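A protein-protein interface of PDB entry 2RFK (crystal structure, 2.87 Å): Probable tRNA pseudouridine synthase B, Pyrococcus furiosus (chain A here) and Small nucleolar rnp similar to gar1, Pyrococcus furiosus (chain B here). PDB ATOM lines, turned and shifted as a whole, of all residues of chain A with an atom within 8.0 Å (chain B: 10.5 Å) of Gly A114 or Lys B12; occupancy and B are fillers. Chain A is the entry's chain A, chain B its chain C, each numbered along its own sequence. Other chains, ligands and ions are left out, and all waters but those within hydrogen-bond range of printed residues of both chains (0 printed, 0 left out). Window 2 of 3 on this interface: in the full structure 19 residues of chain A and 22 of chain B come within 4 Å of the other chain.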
ATOM      1  N   HIS A 111     -13.258  25.995  10.860  1.00  0.00           N
ATOM      2  CA  HIS A 111     -13.632  24.830  11.642  1.00  0.00           C
ATOM      3  C   HIS A 111     -12.624  23.697  11.513  1.00  0.00           C
ATOM      4  O   HIS A 111     -12.131  23.390  10.425  1.00  0.00           O
ATOM      5  CB  HIS A 111     -15.040  24.336  11.351  1.00  0.00           C
ATOM      6  CG  HIS A 111     -15.489  23.284  12.314  1.00  0.00           C
ATOM      7  ND1 HIS A 111     -15.960  23.583  13.574  1.00  0.00           N
ATOM      8  CD2 HIS A 111     -15.477  21.933  12.226  1.00  0.00           C
ATOM      9  CE1 HIS A 111     -16.250  22.462  14.210  1.00  0.00           C
ATOM     10  NE2 HIS A 111     -15.961  21.445  13.416  1.00  0.00           N
ATOM     11  N   LEU A 112     -12.342  23.072  12.644  1.00  0.00           N
ATOM     12  CA  LEU A 112     -11.374  22.009  12.700  1.00  0.00           C
ATOM     13  C   LEU A 112     -12.045  20.652  12.797  1.00  0.00           C
ATOM     14  O   LEU A 112     -13.151  20.524  13.337  1.00  0.00           O
ATOM     15  CB  LEU A 112     -10.446  22.223  13.891  1.00  0.00           C
ATOM     16  CG  LEU A 112      -9.378  23.294  13.705  1.00  0.00           C
ATOM     17  CD1 LEU A 112      -8.708  23.619  15.026  1.00  0.00           C
ATOM     18  CD2 LEU A 112      -8.364  22.817  12.689  1.00  0.00           C
ATOM     19  N   HIS A 113     -11.358  19.642  12.271  1.00  0.00           N
ATOM     20  CA  HIS A 113     -11.811  18.270  12.365  1.00  0.00           C
ATOM     21  C   HIS A 113     -10.973  17.536  13.401  1.00  0.00           C
ATOM     22  O   HIS A 113     -10.399  16.488  13.115  1.00  0.00           O
ATOM     23  CB  HIS A 113     -11.705  17.575  11.004  1.00  0.00           C
ATOM     24  CG  HIS A 113     -12.334  18.337   9.880  1.00  0.00           C
ATOM     25  ND1 HIS A 113     -11.911  18.215   8.576  1.00  0.00           N
ATOM     26  CD2 HIS A 113     -13.351  19.233   9.866  1.00  0.00           C
ATOM     27  CE1 HIS A 113     -12.640  19.003   7.805  1.00  0.00           C
ATOM     28  NE2 HIS A 113     -13.519  19.631   8.564  1.00  0.00           N
ATOM     29  N   GLY A 114     -10.905  18.093  14.608  1.00  0.00           N
ATOM     30  CA  GLY A 114     -10.097  17.504  15.679  1.00  0.00           C
ATOM     31  C   GLY A 114      -9.523  18.537  16.629  1.00  0.00           C
ATOM     32  O   GLY A 114      -9.288  19.689  16.247  1.00  0.00           O
ATOM     33  N   ASP A 115      -9.288  18.122  17.869  1.00  0.00           N
ATOM     34  CA  ASP A 115      -8.903  19.058  18.916  1.00  0.00           C
ATOM     35  C   ASP A 115      -7.403  19.208  19.006  1.00  0.00           C
ATOM     36  O   ASP A 115      -6.684  18.271  19.367  1.00  0.00           O
ATOM     37  CB  ASP A 115      -9.471  18.636  20.274  1.00  0.00           C
ATOM     38  CG  ASP A 115     -10.986  18.532  20.274  1.00  0.00           C
ATOM     39  OD1 ASP A 115     -11.506  17.576  20.890  1.00  0.00           O
ATOM     40  OD2 ASP A 115     -11.654  19.394  19.662  1.00  0.00           O
ATOM     41  N   VAL A 116      -6.939  20.398  18.665  1.00  0.00           N
ATOM     42  CA  VAL A 116      -5.551  20.748  18.854  1.00  0.00           C
ATOM     43  C   VAL A 116      -5.507  21.728  20.014  1.00  0.00           C
ATOM     44  O   VAL A 116      -6.343  22.626  20.089  1.00  0.00           O
ATOM     45  CB  VAL A 116      -4.942  21.394  17.590  1.00  0.00           C
ATOM     46  CG1 VAL A 116      -3.441  21.611  17.759  1.00  0.00           C
ATOM     47  CG2 VAL A 116      -5.217  20.530  16.370  1.00  0.00           C
ATOM     48  N   PRO A 117      -4.560  21.531  20.943  1.00  0.00           N
ATOM     49  CA  PRO A 117      -4.286  22.506  21.992  1.00  0.00           C
ATOM     50  C   PRO A 117      -4.206  23.920  21.424  1.00  0.00           C
ATOM     51  O   PRO A 117      -3.611  24.124  20.363  1.00  0.00           O
ATOM     52  CB  PRO A 117      -2.916  22.078  22.528  1.00  0.00           C
ATOM     53  CG  PRO A 117      -2.486  20.882  21.693  1.00  0.00           C
ATOM     54  CD  PRO A 117      -3.706  20.339  21.066  1.00  0.00           C
ATOM     55  N   ILE A 121      -1.857  26.158  18.273  1.00  0.00           N
ATOM     56  CA  ILE A 121      -2.587  26.618  17.099  1.00  0.00           C
ATOM     57  C   ILE A 121      -2.103  28.003  16.647  1.00  0.00           C
ATOM     58  O   ILE A 121      -1.697  28.170  15.495  1.00  0.00           O
ATOM     59  CB  ILE A 121      -4.117  26.589  17.326  1.00  0.00           C
ATOM     60  CG1 ILE A 121      -4.569  25.143  17.569  1.00  0.00           C
ATOM     61  CG2 ILE A 121      -4.859  27.220  16.141  1.00  0.00           C
ATOM     62  CD1 ILE A 121      -5.934  25.000  18.232  1.00  0.00           C
ATOM     63  N   GLY A 161     -12.402  25.948  21.250  1.00  0.00           N
ATOM     64  CA  GLY A 161     -12.151  24.552  20.867  1.00  0.00           C
ATOM     65  C   GLY A 161     -11.808  24.257  19.410  1.00  0.00           C
ATOM     66  O   GLY A 161     -10.641  24.311  19.017  1.00  0.00           O
ATOM     67  N   ARG A 162     -12.829  23.941  18.614  1.00  0.00           N
ATOM     68  CA  ARG A 162     -12.638  23.506  17.226  1.00  0.00           C
ATOM     69  C   ARG A 162     -12.813  24.618  16.197  1.00  0.00           C
ATOM     70  O   ARG A 162     -12.429  24.462  15.034  1.00  0.00           O
ATOM     71  CB  ARG A 162     -13.584  22.350  16.894  1.00  0.00           C
ATOM     72  CG  ARG A 162     -13.075  20.984  17.302  1.00  0.00           C
ATOM     73  CD  ARG A 162     -13.970  19.904  16.735  1.00  0.00           C
ATOM     74  NE  ARG A 162     -13.303  18.602  16.646  1.00  0.00           N
ATOM     75  CZ  ARG A 162     -13.410  17.637  17.555  1.00  0.00           C
ATOM     76  NH1 ARG A 162     -14.151  17.816  18.639  1.00  0.00           N
ATOM     77  NH2 ARG A 162     -12.776  16.489  17.381  1.00  0.00           N
ATOM     78  N   ASP A 163     -13.402  25.733  16.627  1.00  0.00           N
ATOM     79  CA  ASP A 163     -13.594  26.898  15.762  1.00  0.00           C
ATOM     80  C   ASP A 163     -12.561  28.000  16.015  1.00  0.00           C
ATOM     81  O   ASP A 163     -12.231  28.323  17.161  1.00  0.00           O
ATOM     82  CB  ASP A 163     -15.019  27.434  15.888  1.00  0.00           C
ATOM     83  CG  ASP A 163     -16.043  26.551  15.173  1.00  0.00           C
ATOM     84  OD1 ASP A 163     -15.932  26.382  13.936  1.00  0.00           O
ATOM     85  OD2 ASP A 163     -16.967  26.033  15.845  1.00  0.00           O
ATOM     86  N   VAL A 164     -12.045  28.563  14.927  1.00  0.00           N
ATOM     87  CA  VAL A 164     -10.948  29.521  15.001  1.00  0.00           C
ATOM     88  C   VAL A 164     -11.307  30.751  14.186  1.00  0.00           C
ATOM     89  O   VAL A 164     -11.675  30.654  13.007  1.00  0.00           O
ATOM     90  CB  VAL A 164      -9.600  28.913  14.507  1.00  0.00           C
ATOM     91  CG1 VAL A 164      -8.436  29.801  14.889  1.00  0.00           C
ATOM     92  CG2 VAL A 164      -9.394  27.546  15.097  1.00  0.00           C
ATOM     93  N   GLY A 184      -5.158  23.249   7.776  1.00  0.00           N
ATOM     94  CA  GLY A 184      -5.863  22.043   8.199  1.00  0.00           C
ATOM     95  C   GLY A 184      -4.959  20.845   8.068  1.00  0.00           C
ATOM     96  O   GLY A 184      -4.598  20.227   9.068  1.00  0.00           O
ATOM     97  N   LEU A 185      -4.571  20.544   6.831  1.00  0.00           N
ATOM     98  CA  LEU A 185      -3.601  19.488   6.540  1.00  0.00           C
ATOM     99  C   LEU A 185      -2.408  19.560   7.475  1.00  0.00           C
ATOM    100  O   LEU A 185      -1.958  18.541   7.985  1.00  0.00           O
ATOM    101  CB  LEU A 185      -3.106  19.597   5.092  1.00  0.00           C
ATOM    102  CG  LEU A 185      -3.669  18.766   3.931  1.00  0.00           C
ATOM    103  CD1 LEU A 185      -5.185  18.697   3.935  1.00  0.00           C
ATOM    104  CD2 LEU A 185      -3.160  19.298   2.578  1.00  0.00           C
ATOM    105  N   LEU A 187      -1.939  21.009  10.477  1.00  0.00           N
ATOM    106  CA  LEU A 187      -2.197  20.651  11.861  1.00  0.00           C
ATOM    107  C   LEU A 187      -2.578  19.175  11.978  1.00  0.00           C
ATOM    108  O   LEU A 187      -2.466  18.580  13.053  1.00  0.00           O
ATOM    109  CB  LEU A 187      -3.252  21.573  12.476  1.00  0.00           C
ATOM    110  CG  LEU A 187      -2.704  22.871  13.077  1.00  0.00           C
ATOM    111  CD1 LEU A 187      -3.816  23.890  13.260  1.00  0.00           C
ATOM    112  CD2 LEU A 187      -1.983  22.621  14.404  1.00  0.00           C
ATOM    113  N   GLY A 188      -3.006  18.592  10.857  1.00  0.00           N
ATOM    114  CA  GLY A 188      -3.314  17.160  10.772  1.00  0.00           C
ATOM    115  C   GLY A 188      -4.802  16.879  10.836  1.00  0.00           C
ATOM    116  O   GLY A 188      -5.385  16.287   9.917  1.00  0.00           O
ATOM    117  N   VAL A 189      -5.413  17.322  11.932  1.00  0.00           N
ATOM    118  CA  VAL A 189      -6.838  17.145  12.173  1.00  0.00           C
ATOM    119  C   VAL A 189      -7.661  17.437  10.915  1.00  0.00           C
ATOM    120  O   VAL A 189      -8.597  16.704  10.591  1.00  0.00           O
ATOM    121  CB  VAL A 189      -7.318  17.991  13.382  1.00  0.00           C
ATOM    122  CG1 VAL A 189      -6.739  17.449  14.679  1.00  0.00           C
ATOM    123  CG2 VAL A 189      -6.935  19.443  13.217  1.00  0.00           C
ATOM    124  N   GLY A 190      -7.271  18.476  10.185  1.00  0.00           N
ATOM    125  CA  GLY A 190      -7.978  18.874   8.984  1.00  0.00           C
ATOM    126  C   GLY A 190      -8.956  19.982   9.312  1.00  0.00           C
ATOM    127  O   GLY A 190      -9.543  20.020  10.402  1.00  0.00           O
ATOM    128  N   ALA A 191      -9.134  20.894   8.368  1.00  0.00           N
ATOM    129  CA  ALA A 191     -10.008  22.018   8.586  1.00  0.00           C
ATOM    130  C   ALA A 191     -10.716  22.436   7.306  1.00  0.00           C
ATOM    131  O   ALA A 191     -10.432  21.897   6.223  1.00  0.00           O
ATOM    132  CB  ALA A 191      -9.219  23.178   9.166  1.00  0.00           C
ATOM    133  N   LEU B   8       6.058  14.633  11.491  1.00  0.00           N
ATOM    134  CA  LEU B   8       5.471  15.325  12.639  1.00  0.00           C
ATOM    135  C   LEU B   8       4.210  14.632  13.156  1.00  0.00           C
ATOM    136  O   LEU B   8       3.975  14.585  14.370  1.00  0.00           O
ATOM    137  CB  LEU B   8       5.201  16.800  12.298  1.00  0.00           C
ATOM    138  CG  LEU B   8       6.268  17.854  12.643  1.00  0.00           C
ATOM    139  CD1 LEU B   8       7.638  17.567  12.030  1.00  0.00           C
ATOM    140  CD2 LEU B   8       5.803  19.240  12.232  1.00  0.00           C
ATOM    141  N   HIS B   9       3.406  14.111  12.228  1.00  0.00           N
ATOM    142  CA  HIS B   9       2.213  13.306  12.533  1.00  0.00           C
ATOM    143  C   HIS B   9       1.541  12.779  11.263  1.00  0.00           C
ATOM    144  O   HIS B   9       2.072  12.927  10.154  1.00  0.00           O
ATOM    145  CB  HIS B   9       1.192  14.071  13.401  1.00  0.00           C
ATOM    146  CG  HIS B   9       1.192  15.553  13.187  1.00  0.00           C
ATOM    147  ND1 HIS B   9       0.946  16.131  11.960  1.00  0.00           N
ATOM    148  CD2 HIS B   9       1.409  16.575  14.048  1.00  0.00           C
ATOM    149  CE1 HIS B   9       1.014  17.445  12.074  1.00  0.00           C
ATOM    150  NE2 HIS B   9       1.295  17.740  13.331  1.00  0.00           N
ATOM    151  N   TYR B  10       0.384  12.147  11.446  1.00  0.00           N
ATOM    152  CA  TYR B  10      -0.450  11.680  10.345  1.00  0.00           C
ATOM    153  C   TYR B  10      -1.715  12.528  10.277  1.00  0.00           C
ATOM    154  O   TYR B  10      -2.398  12.720  11.286  1.00  0.00           O
ATOM    155  CB  TYR B  10      -0.793  10.191  10.521  1.00  0.00           C
ATOM    156  CG  TYR B  10      -1.557   9.558   9.366  1.00  0.00           C
ATOM    157  CD1 TYR B  10      -1.257   9.876   8.037  1.00  0.00           C
ATOM    158  CD2 TYR B  10      -2.564   8.613   9.600  1.00  0.00           C
ATOM    159  CE1 TYR B  10      -1.951   9.295   6.974  1.00  0.00           C
ATOM    160  CE2 TYR B  10      -3.264   8.020   8.539  1.00  0.00           C
ATOM    161  CZ  TYR B  10      -2.950   8.372   7.230  1.00  0.00           C
ATOM    162  OH  TYR B  10      -3.626   7.801   6.174  1.00  0.00           O
ATOM    163  N   ALA B  11      -2.012  13.053   9.090  1.00  0.00           N
ATOM    164  CA  ALA B  11      -3.213  13.858   8.892  1.00  0.00           C
ATOM    165  C   ALA B  11      -4.409  12.935   8.794  1.00  0.00           C
ATOM    166  O   ALA B  11      -4.357  11.905   8.104  1.00  0.00           O
ATOM    167  CB  ALA B  11      -3.095  14.717   7.652  1.00  0.00           C
ATOM    168  N   LYS B  12      -5.478  13.319   9.491  1.00  0.00           N
ATOM    169  CA  LYS B  12      -6.696  12.510   9.627  1.00  0.00           C
ATOM    170  C   LYS B  12      -7.410  12.288   8.291  1.00  0.00           C
ATOM    171  O   LYS B  12      -8.352  11.501   8.203  1.00  0.00           O
ATOM    172  CB  LYS B  12      -7.658  13.151  10.641  1.00  0.00           C
ATOM    173  CG  LYS B  12      -7.162  13.195  12.095  1.00  0.00           C
ATOM    174  CD  LYS B  12      -8.245  13.745  13.035  1.00  0.00           C
ATOM    175  CE  LYS B  12      -7.789  13.768  14.495  1.00  0.00           C
ATOM    176  NZ  LYS B  12      -8.863  14.244  15.424  1.00  0.00           N
ATOM    177  N   GLN B  13      -6.956  12.984   7.256  1.00  0.00           N
ATOM    178  CA  GLN B  13      -7.567  12.880   5.939  1.00  0.00           C
ATOM    179  C   GLN B  13      -6.832  11.867   5.058  1.00  0.00           C
ATOM    180  O   GLN B  13      -7.430  11.278   4.153  1.00  0.00           O
ATOM    181  CB  GLN B  13      -7.673  14.263   5.296  1.00  0.00           C
ATOM    182  CG  GLN B  13      -8.695  15.169   6.011  1.00  0.00           C
ATOM    183  CD  GLN B  13      -8.538  16.645   5.676  1.00  0.00           C
ATOM    184  OE1 GLN B  13      -7.693  17.032   4.863  1.00  0.00           O
ATOM    185  NE2 GLN B  13      -9.362  17.484   6.307  1.00  0.00           N
ATOM    186  N   GLY B  14      -5.548  11.655   5.342  1.00  0.00           N
ATOM    187  CA  GLY B  14      -4.802  10.560   4.738  1.00  0.00           C
ATOM    188  C   GLY B  14      -3.406  10.891   4.252  1.00  0.00           C
ATOM    189  O   GLY B  14      -2.961  10.349   3.233  1.00  0.00           O
ATOM    190  N   PHE B  15      -2.709  11.761   4.987  1.00  0.00           N
ATOM    191  CA  PHE B  15      -1.390  12.261   4.564  1.00  0.00           C
ATOM    192  C   PHE B  15      -0.311  12.292   5.650  1.00  0.00           C
ATOM    193  O   PHE B  15      -0.551  12.743   6.770  1.00  0.00           O
ATOM    194  CB  PHE B  15      -1.523  13.661   3.959  1.00  0.00           C
ATOM    195  CG  PHE B  15      -1.990  13.669   2.530  1.00  0.00           C
ATOM    196  CD1 PHE B  15      -3.234  13.140   2.173  1.00  0.00           C
ATOM    197  CD2 PHE B  15      -1.202  14.241   1.540  1.00  0.00           C
ATOM    198  CE1 PHE B  15      -3.674  13.156   0.854  1.00  0.00           C
ATOM    199  CE2 PHE B  15      -1.628  14.267   0.216  1.00  0.00           C
ATOM    200  CZ  PHE B  15      -2.874  13.727  -0.129  1.00  0.00           C
ATOM    201  N   LEU B  16       0.884  11.822   5.301  1.00  0.00           N
ATOM    202  CA  LEU B  16       2.048  11.946   6.175  1.00  0.00           C
ATOM    203  C   LEU B  16       2.583  13.357   6.064  1.00  0.00           C
ATOM    204  O   LEU B  16       2.806  13.854   4.953  1.00  0.00           O
ATOM    205  CB  LEU B  16       3.161  10.977   5.766  1.00  0.00           C
ATOM    206  CG  LEU B  16       3.050   9.474   5.996  1.00  0.00           C
ATOM    207  CD1 LEU B  16       2.195   8.821   4.937  1.00  0.00           C
ATOM    208  CD2 LEU B  16       4.434   8.873   5.967  1.00  0.00           C
ATOM    209  N   ILE B  17       2.802  13.996   7.211  1.00  0.00           N
ATOM    210  CA  ILE B  17       3.336  15.356   7.223  1.00  0.00           C
ATOM    211  C   ILE B  17       4.781  15.388   7.699  1.00  0.00           C
ATOM    212  O   ILE B  17       5.060  15.315   8.900  1.00  0.00           O
ATOM    213  CB  ILE B  17       2.498  16.340   8.069  1.00  0.00           C
ATOM    214  CG1 ILE B  17       1.008  16.229   7.743  1.00  0.00           C
ATOM    215  CG2 ILE B  17       2.982  17.755   7.845  1.00  0.00           C
ATOM    216  CD1 ILE B  17       0.244  15.401   8.739  1.00  0.00           C
ATOM    217  N   ALA B  54       3.261  17.468   2.212  1.00  0.00           N
ATOM    218  CA  ALA B  54       2.172  16.530   2.524  1.00  0.00           C
ATOM    219  C   ALA B  54       2.221  15.295   1.623  1.00  0.00           C
ATOM    220  O   ALA B  54       2.229  15.417   0.393  1.00  0.00           O
ATOM    221  CB  ALA B  54       0.827  17.205   2.418  1.00  0.00           C
ATOM    222  N   ILE B  55       2.233  14.115   2.248  1.00  0.00           N
ATOM    223  CA  ILE B  55       2.355  12.844   1.528  1.00  0.00           C
ATOM    224  C   ILE B  55       1.069  12.014   1.528  1.00  0.00           C
ATOM    225  O   ILE B  55       0.509  11.734   2.586  1.00  0.00           O
ATOM    226  CB  ILE B  55       3.526  11.980   2.092  1.00  0.00           C
ATOM    227  CG1 ILE B  55       4.881  12.454   1.554  1.00  0.00           C
ATOM    228  CG2 ILE B  55       3.349  10.509   1.738  1.00  0.00           C
ATOM    229  CD1 ILE B  55       5.436  13.702   2.229  1.00  0.00           C
ATOM    230  N   PRO B  57       0.121   8.401   1.070  1.00  0.00           N
ATOM    231  CA  PRO B  57       0.742   7.074   1.078  1.00  0.00           C
ATOM    232  C   PRO B  57       0.005   6.052   0.202  1.00  0.00           C
ATOM    233  O   PRO B  57      -1.169   6.266  -0.137  1.00  0.00           O
ATOM    234  CB  PRO B  57       0.648   6.663   2.549  1.00  0.00           C
ATOM    235  CG  PRO B  57      -0.562   7.364   3.045  1.00  0.00           C
ATOM    236  CD  PRO B  57      -0.573   8.682   2.341  1.00  0.00           C
ATOM    237  N   PRO B  62      -0.414   3.284   7.315  1.00  0.00           N
ATOM    238  CA  PRO B  62       0.064   4.649   7.247  1.00  0.00           C
ATOM    239  C   PRO B  62       0.824   5.098   8.494  1.00  0.00           C
ATOM    240  O   PRO B  62       1.947   5.577   8.389  1.00  0.00           O
ATOM    241  CB  PRO B  62      -1.235   5.450   7.100  1.00  0.00           C
ATOM    242  CG  PRO B  62      -2.378   4.478   7.531  1.00  0.00           C
ATOM    243  CD  PRO B  62      -1.737   3.199   7.956  1.00  0.00           C
ATOM    244  N   GLU B  63       0.214   4.913   9.661  1.00  0.00           N
ATOM    245  CA  GLU B  63       0.622   5.585  10.895  1.00  0.00           C
ATOM    246  C   GLU B  63       1.978   5.145  11.463  1.00  0.00           C
ATOM    247  O   GLU B  63       2.510   5.788  12.370  1.00  0.00           O
ATOM    248  CB  GLU B  63      -0.478   5.417  11.949  1.00  0.00           C
ATOM    249  CG  GLU B  63      -0.697   6.629  12.844  1.00  0.00           C
ATOM    250  CD  GLU B  63      -1.822   6.418  13.846  1.00  0.00           C
ATOM    251  OE1 GLU B  63      -1.989   5.272  14.324  1.00  0.00           O
ATOM    252  OE2 GLU B  63      -2.540   7.392  14.163  1.00  0.00           O
ATOM    253  N   VAL B  66       5.251   7.951  12.132  1.00  0.00           N
ATOM    254  CA  VAL B  66       5.316   9.066  13.097  1.00  0.00           C
ATOM    255  C   VAL B  66       6.655   9.128  13.835  1.00  0.00           C
ATOM    256  O   VAL B  66       7.022   8.200  14.561  1.00  0.00           O
ATOM    257  CB  VAL B  66       4.145   9.029  14.122  1.00  0.00           C
ATOM    258  CG1 VAL B  66       4.272  10.161  15.139  1.00  0.00           C
ATOM    259  CG2 VAL B  66       2.806   9.115  13.414  1.00  0.00           C
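A ring nitrogen (ND1) of His A113 lies within hydrogen-bond range of the side-chain amide nitrogen (NE2) of Gln B13 (3.5 Å). The backbone NH of Lys B12 lies within hydrogen-bond range of the backbone carbonyl oxygen of Gly A188 (3.0 Å).
O of Gly A190 is in hydrogen-bond range of N of His A113 (2.6 Å). O of Gly A184 is in hydrogen-bond range of N of Gly A190. The backbone NH (N) of Leu B8 is in hydrogen-bond range of the backbone carbonyl oxygen (O) of Ile B17, at 2.9 Å. The backbone carbonyl oxygen of His B9 sits at hydrogen-bond distance from the backbone NH of Ile B17 (3.2 Å).
Among the printed residues, pairs that only touch across the chains: His A113 with Lys B12, Gly A114 with Lys B12, Leu A185 with Gln B13, Leu A185 with Ile B17, Leu A187 with His B9, Gly A188 with Ala B11, Val A189 with Lys B12, Gly A190 with Gln B13 and Ala A191 with Gln B13.
Leu A112 touches none of the printed residues of chain B. Val A116 touches none of the printed residues of chain B. No residue of chain B comes within 4 Å of Arg A162. Printed residues of chain B within 4 Å of Leu A185: Gln B13 (3.2 Å) and Ile B17 (3.8 Å). Gly A188 touches two residues of chain B. Val A189 touches one residue of chain B. Gly A190 touches just one residue of chain B: Gln B13 (3.3 Å). Of the printed residues of chain B, Ala A191 touches Gln B13 (3.99 Å). Printed residues of chain A within 4 Å of Ala B11: Gly A188 (3.4 Å). Of chain A, only His A113, Gly A114, Gly A188 and Val A189 come within 4 Å of Lys B12. Printed residues of chain A within 4 Å of Gln B13: His A113, Leu A185, Gly A190 and Ala A191. Of the printed residues of chain A, Ile B17 touches Leu A185. Ala B54 touches none of the printed residues of chain A. The nearest residue of chain B that does not touch Gly A114 is Gln B13 (8.5 Å). The nearest residue of chain A that does not touch Lys B12 is Asp A115 (4.6 Å). The nearest printed residue of chain B that does not touch His A113 is Ala B11 (8.2 Å).
Of the 16 printed residues of chain B, 5 touch a printed residue of chain A. Hydrophobic or aromatic side chains of chain B that line the printed part of chain A: His B9, Ala B11 and Ile B17. Of the 19 printed residues of chain A, 8 touch a printed residue of chain B. Hydrophobic or aromatic side chains of chain A within 4 Å of the printed part of chain B: His A113, Leu A185 and Val A189. Among the printed residues, no Asp or Glu carboxylate lies within 4 Å of a Lys or Arg side-chain nitrogen of the other chain.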
